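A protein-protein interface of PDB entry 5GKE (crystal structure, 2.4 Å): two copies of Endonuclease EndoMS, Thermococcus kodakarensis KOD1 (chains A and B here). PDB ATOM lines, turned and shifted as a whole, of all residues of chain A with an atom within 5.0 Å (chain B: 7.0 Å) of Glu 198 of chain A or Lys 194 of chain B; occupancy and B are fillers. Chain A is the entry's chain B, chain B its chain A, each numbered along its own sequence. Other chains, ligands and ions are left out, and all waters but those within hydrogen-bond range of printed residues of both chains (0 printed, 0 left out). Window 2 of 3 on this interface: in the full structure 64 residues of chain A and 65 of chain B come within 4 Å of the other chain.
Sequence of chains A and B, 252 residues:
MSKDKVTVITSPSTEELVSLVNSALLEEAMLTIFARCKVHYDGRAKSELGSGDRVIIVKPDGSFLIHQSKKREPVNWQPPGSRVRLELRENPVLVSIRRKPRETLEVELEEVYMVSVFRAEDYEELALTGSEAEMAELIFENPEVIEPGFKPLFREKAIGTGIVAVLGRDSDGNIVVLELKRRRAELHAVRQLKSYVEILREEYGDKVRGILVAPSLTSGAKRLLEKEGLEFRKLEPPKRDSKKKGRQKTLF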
ATOM      1  N   LYS A 194     -30.338  29.850  -2.180  1.00  0.00           N
ATOM      2  CA  LYS A 194     -30.943  30.145  -0.896  1.00  0.00           C
ATOM      3  C   LYS A 194     -30.047  31.072  -0.088  1.00  0.00           C
ATOM      4  O   LYS A 194     -30.516  31.946   0.651  1.00  0.00           O
ATOM      5  CB  LYS A 194     -31.212  28.847  -0.139  1.00  0.00           C
ATOM      6  CG  LYS A 194     -31.553  29.026   1.321  1.00  0.00           C
ATOM      7  CD  LYS A 194     -31.786  27.683   1.986  1.00  0.00           C
ATOM      8  CE  LYS A 194     -32.285  27.841   3.410  1.00  0.00           C
ATOM      9  NZ  LYS A 194     -31.280  28.456   4.315  1.00  0.00           N
ATOM     10  N   SER A 195     -28.747  30.893  -0.257  1.00  0.00           N
ATOM     11  CA  SER A 195     -27.784  31.683   0.483  1.00  0.00           C
ATOM     12  C   SER A 195     -27.771  33.130   0.044  1.00  0.00           C
ATOM     13  O   SER A 195     -27.652  34.022   0.863  1.00  0.00           O
ATOM     14  CB  SER A 195     -26.386  31.114   0.315  1.00  0.00           C
ATOM     15  OG  SER A 195     -25.518  31.761   1.211  1.00  0.00           O
ATOM     16  N   TYR A 196     -27.833  33.341  -1.264  1.00  0.00           N
ATOM     17  CA  TYR A 196     -27.824  34.680  -1.831  1.00  0.00           C
ATOM     18  C   TYR A 196     -29.092  35.415  -1.410  1.00  0.00           C
ATOM     19  O   TYR A 196     -29.041  36.555  -0.953  1.00  0.00           O
ATOM     20  CB  TYR A 196     -27.720  34.619  -3.362  1.00  0.00           C
ATOM     21  CG  TYR A 196     -26.491  33.892  -3.872  1.00  0.00           C
ATOM     22  CD1 TYR A 196     -25.306  33.908  -3.153  1.00  0.00           C
ATOM     23  CD2 TYR A 196     -26.519  33.198  -5.073  1.00  0.00           C
ATOM     24  CE1 TYR A 196     -24.182  33.259  -3.611  1.00  0.00           C
ATOM     25  CE2 TYR A 196     -25.388  32.539  -5.545  1.00  0.00           C
ATOM     26  CZ  TYR A 196     -24.226  32.569  -4.805  1.00  0.00           C
ATOM     27  OH  TYR A 196     -23.097  31.920  -5.266  1.00  0.00           O
ATOM     28  N   VAL A 197     -30.222  34.730  -1.555  1.00  0.00           N
ATOM     29  CA  VAL A 197     -31.530  35.286  -1.264  1.00  0.00           C
ATOM     30  C   VAL A 197     -31.654  35.747   0.187  1.00  0.00           C
ATOM     31  O   VAL A 197     -32.127  36.844   0.458  1.00  0.00           O
ATOM     32  CB  VAL A 197     -32.623  34.271  -1.560  1.00  0.00           C
ATOM     33  CG1 VAL A 197     -33.972  34.775  -1.019  1.00  0.00           C
ATOM     34  CG2 VAL A 197     -32.688  34.008  -3.056  1.00  0.00           C
ATOM     35  N   GLU A 198     -31.206  34.914   1.114  1.00  0.00           N
ATOM     36  CA  GLU A 198     -31.268  35.268   2.521  1.00  0.00           C
ATOM     37  C   GLU A 198     -30.501  36.543   2.794  1.00  0.00           C
ATOM     38  O   GLU A 198     -30.992  37.443   3.478  1.00  0.00           O
ATOM     39  CB  GLU A 198     -30.714  34.135   3.388  1.00  0.00           C
ATOM     40  CG  GLU A 198     -31.652  32.951   3.489  1.00  0.00           C
ATOM     41  CD  GLU A 198     -31.114  31.869   4.389  1.00  0.00           C
ATOM     42  OE1 GLU A 198     -31.819  30.852   4.590  1.00  0.00           O
ATOM     43  OE2 GLU A 198     -29.986  32.046   4.896  1.00  0.00           O
ATOM     44  N   ILE A 199     -29.283  36.602   2.268  1.00  0.00           N
ATOM     45  CA  ILE A 199     -28.422  37.764   2.430  1.00  0.00           C
ATOM     46  C   ILE A 199     -29.106  39.042   1.908  1.00  0.00           C
ATOM     47  O   ILE A 199     -29.103  40.077   2.565  1.00  0.00           O
ATOM     48  CB  ILE A 199     -27.083  37.506   1.720  1.00  0.00           C
ATOM     49  CG1 ILE A 199     -26.236  36.570   2.583  1.00  0.00           C
ATOM     50  CG2 ILE A 199     -26.330  38.782   1.439  1.00  0.00           C
ATOM     51  CD1 ILE A 199     -24.880  36.319   2.032  1.00  0.00           C
ATOM     52  N   LEU A 200     -29.724  38.939   0.741  1.00  0.00           N
ATOM     53  CA  LEU A 200     -30.434  40.043   0.129  1.00  0.00           C
ATOM     54  C   LEU A 200     -31.738  40.387   0.852  1.00  0.00           C
ATOM     55  O   LEU A 200     -32.126  41.549   0.904  1.00  0.00           O
ATOM     56  CB  LEU A 200     -30.719  39.718  -1.334  1.00  0.00           C
ATOM     57  CG  LEU A 200     -29.453  39.882  -2.177  1.00  0.00           C
ATOM     58  CD1 LEU A 200     -29.630  39.374  -3.600  1.00  0.00           C
ATOM     59  CD2 LEU A 200     -29.070  41.339  -2.170  1.00  0.00           C
ATOM     60  N   ARG A 201     -32.416  39.379   1.394  1.00  0.00           N
ATOM     61  CA  ARG A 201     -33.658  39.605   2.124  1.00  0.00           C
ATOM     62  C   ARG A 201     -33.399  40.458   3.351  1.00  0.00           C
ATOM     63  O   ARG A 201     -34.225  41.285   3.741  1.00  0.00           O
ATOM     64  CB  ARG A 201     -34.307  38.286   2.531  1.00  0.00           C
ATOM     65  CG  ARG A 201     -34.987  37.530   1.398  1.00  0.00           C
ATOM     66  CD  ARG A 201     -36.195  36.800   1.925  1.00  0.00           C
ATOM     67  NE  ARG A 201     -36.269  35.373   1.602  1.00  0.00           N
ATOM     68  CZ  ARG A 201     -36.909  34.876   0.544  1.00  0.00           C
ATOM     69  NH1 ARG A 201     -37.482  35.701  -0.322  1.00  0.00           N
ATOM     70  NH2 ARG A 201     -36.957  33.561   0.337  1.00  0.00           N
ATOM     71  N   GLU A 202     -32.214  40.269   3.917  1.00  0.00           N
ATOM     72  CA  GLU A 202     -31.729  40.981   5.097  1.00  0.00           C
ATOM     73  C   GLU A 202     -31.613  42.495   4.850  1.00  0.00           C
ATOM     74  O   GLU A 202     -31.374  43.281   5.767  1.00  0.00           O
ATOM     75  CB  GLU A 202     -30.364  40.396   5.495  1.00  0.00           C
ATOM     76  CG  GLU A 202     -29.890  40.665   6.913  1.00  0.00           C
ATOM     77  CD  GLU A 202     -28.495  40.102   7.166  1.00  0.00           C
ATOM     78  OE1 GLU A 202     -27.843  39.653   6.191  1.00  0.00           O
ATOM     79  OE2 GLU A 202     -28.053  40.108   8.337  1.00  0.00           O
ATOM     80  N   GLU A 228     -38.173  26.277   0.942  1.00  0.00           N
ATOM     81  CA  GLU A 228     -37.659  27.631   1.154  1.00  0.00           C
ATOM     82  C   GLU A 228     -38.391  28.727   0.362  1.00  0.00           C
ATOM     83  O   GLU A 228     -38.046  29.912   0.463  1.00  0.00           O
ATOM     84  CB  GLU A 228     -36.164  27.669   0.830  1.00  0.00           C
ATOM     85  CG  GLU A 228     -35.327  26.753   1.711  1.00  0.00           C
ATOM     86  CD  GLU A 228     -35.443  27.070   3.203  1.00  0.00           C
ATOM     87  OE1 GLU A 228     -35.801  28.213   3.565  1.00  0.00           O
ATOM     88  OE2 GLU A 228     -35.152  26.168   4.020  1.00  0.00           O
ATOM     89  N   GLU B 179     -18.827  19.389   9.677  1.00  0.00           N
ATOM     90  CA  GLU B 179     -18.485  19.442   8.260  1.00  0.00           C
ATOM     91  C   GLU B 179     -16.959  19.467   8.127  1.00  0.00           C
ATOM     92  O   GLU B 179     -16.294  20.324   8.708  1.00  0.00           O
ATOM     93  CB  GLU B 179     -19.116  20.655   7.578  1.00  0.00           C
ATOM     94  CG  GLU B 179     -18.697  20.838   6.110  1.00  0.00           C
ATOM     95  CD  GLU B 179     -19.132  19.698   5.190  1.00  0.00           C
ATOM     96  OE1 GLU B 179     -18.667  19.662   4.029  1.00  0.00           O
ATOM     97  OE2 GLU B 179     -19.951  18.845   5.607  1.00  0.00           O
ATOM     98  N   ALA B 189     -18.491  25.251   1.829  1.00  0.00           N
ATOM     99  CA  ALA B 189     -18.494  24.368   2.993  1.00  0.00           C
ATOM    100  C   ALA B 189     -19.446  24.872   4.064  1.00  0.00           C
ATOM    101  O   ALA B 189     -20.175  24.084   4.673  1.00  0.00           O
ATOM    102  CB  ALA B 189     -17.091  24.220   3.574  1.00  0.00           C
ATOM    103  N   VAL B 190     -19.435  26.182   4.291  1.00  0.00           N
ATOM    104  CA  VAL B 190     -20.245  26.774   5.349  1.00  0.00           C
ATOM    105  C   VAL B 190     -21.728  26.702   4.993  1.00  0.00           C
ATOM    106  O   VAL B 190     -22.573  26.525   5.869  1.00  0.00           O
ATOM    107  CB  VAL B 190     -19.811  28.223   5.630  1.00  0.00           C
ATOM    108  CG1 VAL B 190     -20.526  28.751   6.833  1.00  0.00           C
ATOM    109  CG2 VAL B 190     -18.294  28.263   5.907  1.00  0.00           C
ATOM    110  N   ARG B 191     -22.022  26.792   3.700  1.00  0.00           N
ATOM    111  CA  ARG B 191     -23.370  26.646   3.179  1.00  0.00           C
ATOM    112  C   ARG B 191     -23.883  25.237   3.403  1.00  0.00           C
ATOM    113  O   ARG B 191     -25.050  25.045   3.720  1.00  0.00           O
ATOM    114  CB  ARG B 191     -23.429  26.970   1.677  1.00  0.00           C
ATOM    115  CG  ARG B 191     -23.127  28.402   1.313  1.00  0.00           C
ATOM    116  CD  ARG B 191     -23.617  28.735  -0.095  1.00  0.00           C
ATOM    117  NE  ARG B 191     -23.095  30.030  -0.504  1.00  0.00           N
ATOM    118  CZ  ARG B 191     -22.075  30.214  -1.340  1.00  0.00           C
ATOM    119  NH1 ARG B 191     -21.465  29.180  -1.912  1.00  0.00           N
ATOM    120  NH2 ARG B 191     -21.679  31.449  -1.619  1.00  0.00           N
ATOM    121  N   GLN B 192     -23.012  24.254   3.185  1.00  0.00           N
ATOM    122  CA  GLN B 192     -23.313  22.870   3.522  1.00  0.00           C
ATOM    123  C   GLN B 192     -23.670  22.753   5.013  1.00  0.00           C
ATOM    124  O   GLN B 192     -24.757  22.315   5.371  1.00  0.00           O
ATOM    125  CB  GLN B 192     -22.116  21.974   3.200  1.00  0.00           C
ATOM    126  CG  GLN B 192     -22.242  21.133   1.940  1.00  0.00           C
ATOM    127  CD  GLN B 192     -20.964  20.330   1.663  1.00  0.00           C
ATOM    128  OE1 GLN B 192     -20.817  19.158   2.071  1.00  0.00           O
ATOM    129  NE2 GLN B 192     -20.034  20.964   0.985  1.00  0.00           N
ATOM    130  N   LEU B 193     -22.738  23.174   5.865  1.00  0.00           N
ATOM    131  CA  LEU B 193     -22.902  23.136   7.305  1.00  0.00           C
ATOM    132  C   LEU B 193     -24.183  23.837   7.784  1.00  0.00           C
ATOM    133  O   LEU B 193     -24.941  23.274   8.551  1.00  0.00           O
ATOM    134  CB  LEU B 193     -21.684  23.770   7.982  1.00  0.00           C
ATOM    135  CG  LEU B 193     -21.719  23.735   9.518  1.00  0.00           C
ATOM    136  CD1 LEU B 193     -21.913  22.300  10.000  1.00  0.00           C
ATOM    137  CD2 LEU B 193     -20.456  24.343  10.144  1.00  0.00           C
ATOM    138  N   LYS B 194     -24.402  25.070   7.342  1.00  0.00           N
ATOM    139  CA  LYS B 194     -25.576  25.830   7.731  1.00  0.00           C
ATOM    140  C   LYS B 194     -26.833  25.079   7.324  1.00  0.00           C
ATOM    141  O   LYS B 194     -27.787  24.963   8.089  1.00  0.00           O
ATOM    142  CB  LYS B 194     -25.544  27.226   7.088  1.00  0.00           C
ATOM    143  CG  LYS B 194     -26.836  28.043   7.184  1.00  0.00           C
ATOM    144  CD  LYS B 194     -26.581  29.489   6.762  1.00  0.00           C
ATOM    145  CE  LYS B 194     -27.789  30.392   6.980  1.00  0.00           C
ATOM    146  NZ  LYS B 194     -28.897  30.110   6.048  1.00  0.00           N
ATOM    147  N   SER B 195     -26.817  24.564   6.107  1.00  0.00           N
ATOM    148  CA  SER B 195     -27.937  23.805   5.590  1.00  0.00           C
ATOM    149  C   SER B 195     -28.270  22.592   6.474  1.00  0.00           C
ATOM    150  O   SER B 195     -29.445  22.293   6.727  1.00  0.00           O
ATOM    151  CB  SER B 195     -27.637  23.361   4.159  1.00  0.00           C
ATOM    152  OG  SER B 195     -28.768  22.788   3.545  1.00  0.00           O
ATOM    153  N   TYR B 196     -27.244  21.901   6.962  1.00  0.00           N
ATOM    154  CA  TYR B 196     -27.496  20.689   7.736  1.00  0.00           C
ATOM    155  C   TYR B 196     -28.026  21.056   9.109  1.00  0.00           C
ATOM    156  O   TYR B 196     -28.954  20.431   9.620  1.00  0.00           O
ATOM    157  CB  TYR B 196     -26.237  19.840   7.871  1.00  0.00           C
ATOM    158  CG  TYR B 196     -25.656  19.419   6.548  1.00  0.00           C
ATOM    159  CD1 TYR B 196     -26.483  19.130   5.458  1.00  0.00           C
ATOM    160  CD2 TYR B 196     -24.270  19.315   6.380  1.00  0.00           C
ATOM    161  CE1 TYR B 196     -25.946  18.751   4.240  1.00  0.00           C
ATOM    162  CE2 TYR B 196     -23.720  18.927   5.165  1.00  0.00           C
ATOM    163  CZ  TYR B 196     -24.556  18.657   4.104  1.00  0.00           C
ATOM    164  OH  TYR B 196     -24.002  18.283   2.911  1.00  0.00           O
ATOM    165  N   VAL B 197     -27.421  22.078   9.699  1.00  0.00           N
ATOM    166  CA  VAL B 197     -27.803  22.515  11.022  1.00  0.00           C
ATOM    167  C   VAL B 197     -29.277  22.924  11.045  1.00  0.00           C
ATOM    168  O   VAL B 197     -30.008  22.565  11.965  1.00  0.00           O
ATOM    169  CB  VAL B 197     -26.931  23.672  11.492  1.00  0.00           C
ATOM    170  CG1 VAL B 197     -27.576  24.382  12.689  1.00  0.00           C
ATOM    171  CG2 VAL B 197     -25.546  23.163  11.840  1.00  0.00           C
ATOM    172  N   GLU B 198     -29.710  23.645  10.016  1.00  0.00           N
ATOM    173  CA  GLU B 198     -31.086  24.111   9.954  1.00  0.00           C
ATOM    174  C   GLU B 198     -32.045  22.939   9.859  1.00  0.00           C
ATOM    175  O   GLU B 198     -33.061  22.903  10.550  1.00  0.00           O
ATOM    176  CB  GLU B 198     -31.292  25.060   8.768  1.00  0.00           C
ATOM    177  CG  GLU B 198     -30.742  26.444   9.010  1.00  0.00           C
ATOM    178  CD  GLU B 198     -30.785  27.333   7.778  1.00  0.00           C
ATOM    179  OE1 GLU B 198     -31.385  26.930   6.750  1.00  0.00           O
ATOM    180  OE2 GLU B 198     -30.205  28.441   7.846  1.00  0.00           O
ATOM    181  N   ILE B 199     -31.723  21.978   9.006  1.00  0.00           N
ATOM    182  CA  ILE B 199     -32.588  20.822   8.843  1.00  0.00           C
ATOM    183  C   ILE B 199     -32.688  20.054  10.153  1.00  0.00           C
ATOM    184  O   ILE B 199     -33.771  19.602  10.535  1.00  0.00           O
ATOM    185  CB  ILE B 199     -32.086  19.910   7.721  1.00  0.00           C
ATOM    186  CG1 ILE B 199     -32.368  20.566   6.371  1.00  0.00           C
ATOM    187  CG2 ILE B 199     -32.758  18.547   7.786  1.00  0.00           C
ATOM    188  CD1 ILE B 199     -31.648  19.914   5.234  1.00  0.00           C
ATOM    189  N   LEU B 200     -31.570  19.947  10.863  1.00  0.00           N
ATOM    190  CA  LEU B 200     -31.558  19.249  12.141  1.00  0.00           C
ATOM    191  C   LEU B 200     -32.274  20.047  13.227  1.00  0.00           C
ATOM    192  O   LEU B 200     -32.871  19.464  14.118  1.00  0.00           O
ATOM    193  CB  LEU B 200     -30.131  18.934  12.577  1.00  0.00           C
ATOM    194  CG  LEU B 200     -29.523  17.728  11.855  1.00  0.00           C
ATOM    195  CD1 LEU B 200     -28.063  17.677  12.130  1.00  0.00           C
ATOM    196  CD2 LEU B 200     -30.161  16.427  12.294  1.00  0.00           C
ATOM    197  N   ARG B 201     -32.216  21.373  13.162  1.00  0.00           N
ATOM    198  CA  ARG B 201     -32.940  22.196  14.130  1.00  0.00           C
ATOM    199  C   ARG B 201     -34.452  22.001  14.004  1.00  0.00           C
ATOM    200  O   ARG B 201     -35.170  22.147  14.979  1.00  0.00           O
ATOM    201  CB  ARG B 201     -32.591  23.674  13.975  1.00  0.00           C
ATOM    202  CG  ARG B 201     -31.266  24.029  14.609  1.00  0.00           C
ATOM    203  CD  ARG B 201     -31.064  25.518  14.822  1.00  0.00           C
ATOM    204  NE  ARG B 201     -29.853  25.721  15.622  1.00  0.00           N
ATOM    205  CZ  ARG B 201     -28.823  26.477  15.251  1.00  0.00           C
ATOM    206  NH1 ARG B 201     -28.864  27.136  14.097  1.00  0.00           N
ATOM    207  NH2 ARG B 201     -27.754  26.586  16.039  1.00  0.00           N
ATOM    208  N   GLY B 210     -23.360  23.415  14.899  1.00  0.00           N
ATOM    209  CA  GLY B 210     -22.530  23.119  13.741  1.00  0.00           C
ATOM    210  C   GLY B 210     -21.056  23.392  13.958  1.00  0.00           C
ATOM    211  O   GLY B 210     -20.677  24.425  14.518  1.00  0.00           O
ATOM    212  N   LEU B 224     -19.086  34.260   7.052  1.00  0.00           N
ATOM    213  CA  LEU B 224     -20.382  33.582   7.073  1.00  0.00           C
ATOM    214  C   LEU B 224     -20.559  32.651   8.268  1.00  0.00           C
ATOM    215  O   LEU B 224     -21.658  32.499   8.798  1.00  0.00           O
ATOM    216  CB  LEU B 224     -20.567  32.795   5.792  1.00  0.00           C
ATOM    217  CG  LEU B 224     -21.872  32.028   5.654  1.00  0.00           C
ATOM    218  CD1 LEU B 224     -23.074  32.936   5.915  1.00  0.00           C
ATOM    219  CD2 LEU B 224     -21.931  31.448   4.262  1.00  0.00           C
ATOM    220  N   LYS B 227     -21.239  34.927  11.388  1.00  0.00           N
ATOM    221  CA  LYS B 227     -22.555  35.523  11.263  1.00  0.00           C
ATOM    222  C   LYS B 227     -23.629  34.530  11.677  1.00  0.00           C
ATOM    223  O   LYS B 227     -24.578  34.880  12.344  1.00  0.00           O
ATOM    224  CB  LYS B 227     -22.790  36.009   9.825  1.00  0.00           C
ATOM    225  CG  LYS B 227     -24.267  36.218   9.439  1.00  0.00           C
ATOM    226  CD  LYS B 227     -24.402  36.825   8.033  1.00  0.00           C
ATOM    227  CE  LYS B 227     -25.846  36.790   7.518  1.00  0.00           C
ATOM    228  NZ  LYS B 227     -26.354  35.406   7.220  1.00  0.00           N
ATOM    229  N   GLU B 228     -23.465  33.274  11.307  1.00  0.00           N
ATOM    230  CA  GLU B 228     -24.536  32.315  11.524  1.00  0.00           C
ATOM    231  C   GLU B 228     -24.436  31.612  12.865  1.00  0.00           C
ATOM    232  O   GLU B 228     -25.212  30.709  13.151  1.00  0.00           O
ATOM    233  CB  GLU B 228     -24.553  31.297  10.394  1.00  0.00           C
ATOM    234  CG  GLU B 228     -25.262  31.823   9.175  1.00  0.00           C
ATOM    235  CD  GLU B 228     -26.695  32.169   9.477  1.00  0.00           C
ATOM    236  OE1 GLU B 228     -27.203  33.146   8.884  1.00  0.00           O
ATOM    237  OE2 GLU B 228     -27.318  31.450  10.296  1.00  0.00           O
ATOM    238  N   LEU B 230     -21.843  29.704  13.933  1.00  0.00           N
ATOM    239  CA  LEU B 230     -21.336  28.356  13.715  1.00  0.00           C
ATOM    240  C   LEU B 230     -19.884  28.317  14.171  1.00  0.00           C
ATOM    241  O   LEU B 230     -19.245  29.360  14.269  1.00  0.00           O
ATOM    242  CB  LEU B 230     -21.482  27.949  12.247  1.00  0.00           C
ATOM    243  CG  LEU B 230     -22.920  27.679  11.798  1.00  0.00           C
ATOM    244  CD1 LEU B 230     -22.995  27.380  10.324  1.00  0.00           C
ATOM    245  CD2 LEU B 230     -23.481  26.521  12.568  1.00  0.00           C
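The side-chain amino group of Lys 194 of chain B lies within salt-bridge range of the side-chain carboxylate of Glu 198 of chain A.
The side-chain amino group of Lys 194 of chain A lies within salt-bridge range of the side-chain carboxylate of Glu 198 of chain B, at 2.9 Å.
OG of Ser 195 of chain A is in hydrogen-bond range of NE of Arg 191 of chain B, 3.4 Å away.
NZ of Lys 194 of chain B lies close to NZ of Lys 194 of chain A, at 3.4 Å.
OE1 of Glu 198 of chain A is in salt-bridge range of NZ of Lys 194 of chain A (2.5 Å).
NZ of Lys 194 of chain B lies within salt-bridge range of OE2 of Glu 198 of chain B (2.8 Å).
The side-chain amino group of Lys 227 of chain B lies within salt-bridge range of the side-chain carboxylate of Glu 228 of chain B, 2.9 Å away.
Among the printed residues, merely in contact across the chains: Tyr 196 of chain A with Arg 191 of chain B (3.7 Å) and Glu 202 of chain A with Lys 227 of chain B (3.7 Å).
Of chain B, only Lys 194 comes within 4 Å of Glu 198 of chain A.
Of chain A, only Lys 194 and Glu 198 come within 4 Å of Lys 194 of chain B.
Printed residues of chain B within 4 Å of Tyr 196 of chain A: Arg 191 (3.7 Å).
Printed residues of chain B within 4 Å of Lys 194 of chain A: Lys 194 (3.4 Å) and Glu 198 (2.9 Å).
Of the printed residues of chain A, Glu 198 of chain B touches Lys 194.
The nearest residue of chain B that does not touch Glu 198 of chain A is Glu 198 of chain B (4.4 Å).
The nearest printed residue of chain A that does not touch Lys 194 of chain B is Ser 195 of chain A (5.9 Å).
The nearest printed residue of chain B that does not touch Ser 195 of chain A is Leu 224 of chain B (4.7 Å).
Printed residues of chain A that touch a printed residue of chain B: Lys 194, Ser 195, Tyr 196, Glu 198 and Glu 202.
Hydrophobic or aromatic side chains of chain A that line the printed part of chain B: Tyr 196.
Printed residues of chain B that touch a printed residue of chain A: Arg 191, Lys 194, Glu 198 and Lys 227.
Among the printed residues, Asp or Glu carboxylates within 4 Å of a Lys or Arg side-chain nitrogen of the other chain: Lys 194 of chain A with Glu 198 of chain B (2.9 Å) and Glu 198 of chain A with Lys 194 of chain B (2.5 Å).
Lys 194 of chain B touches its own counterpart, Lys 194 of chain A.
Lys 194 of chain A touches Glu 198 of chain B, and with the chains exchanged Glu 198 of chain A touches Lys 194 of chain B.
Positions printed for both chains: 194, 195, 196, 197, 198, 199, 200, 201 and 228.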
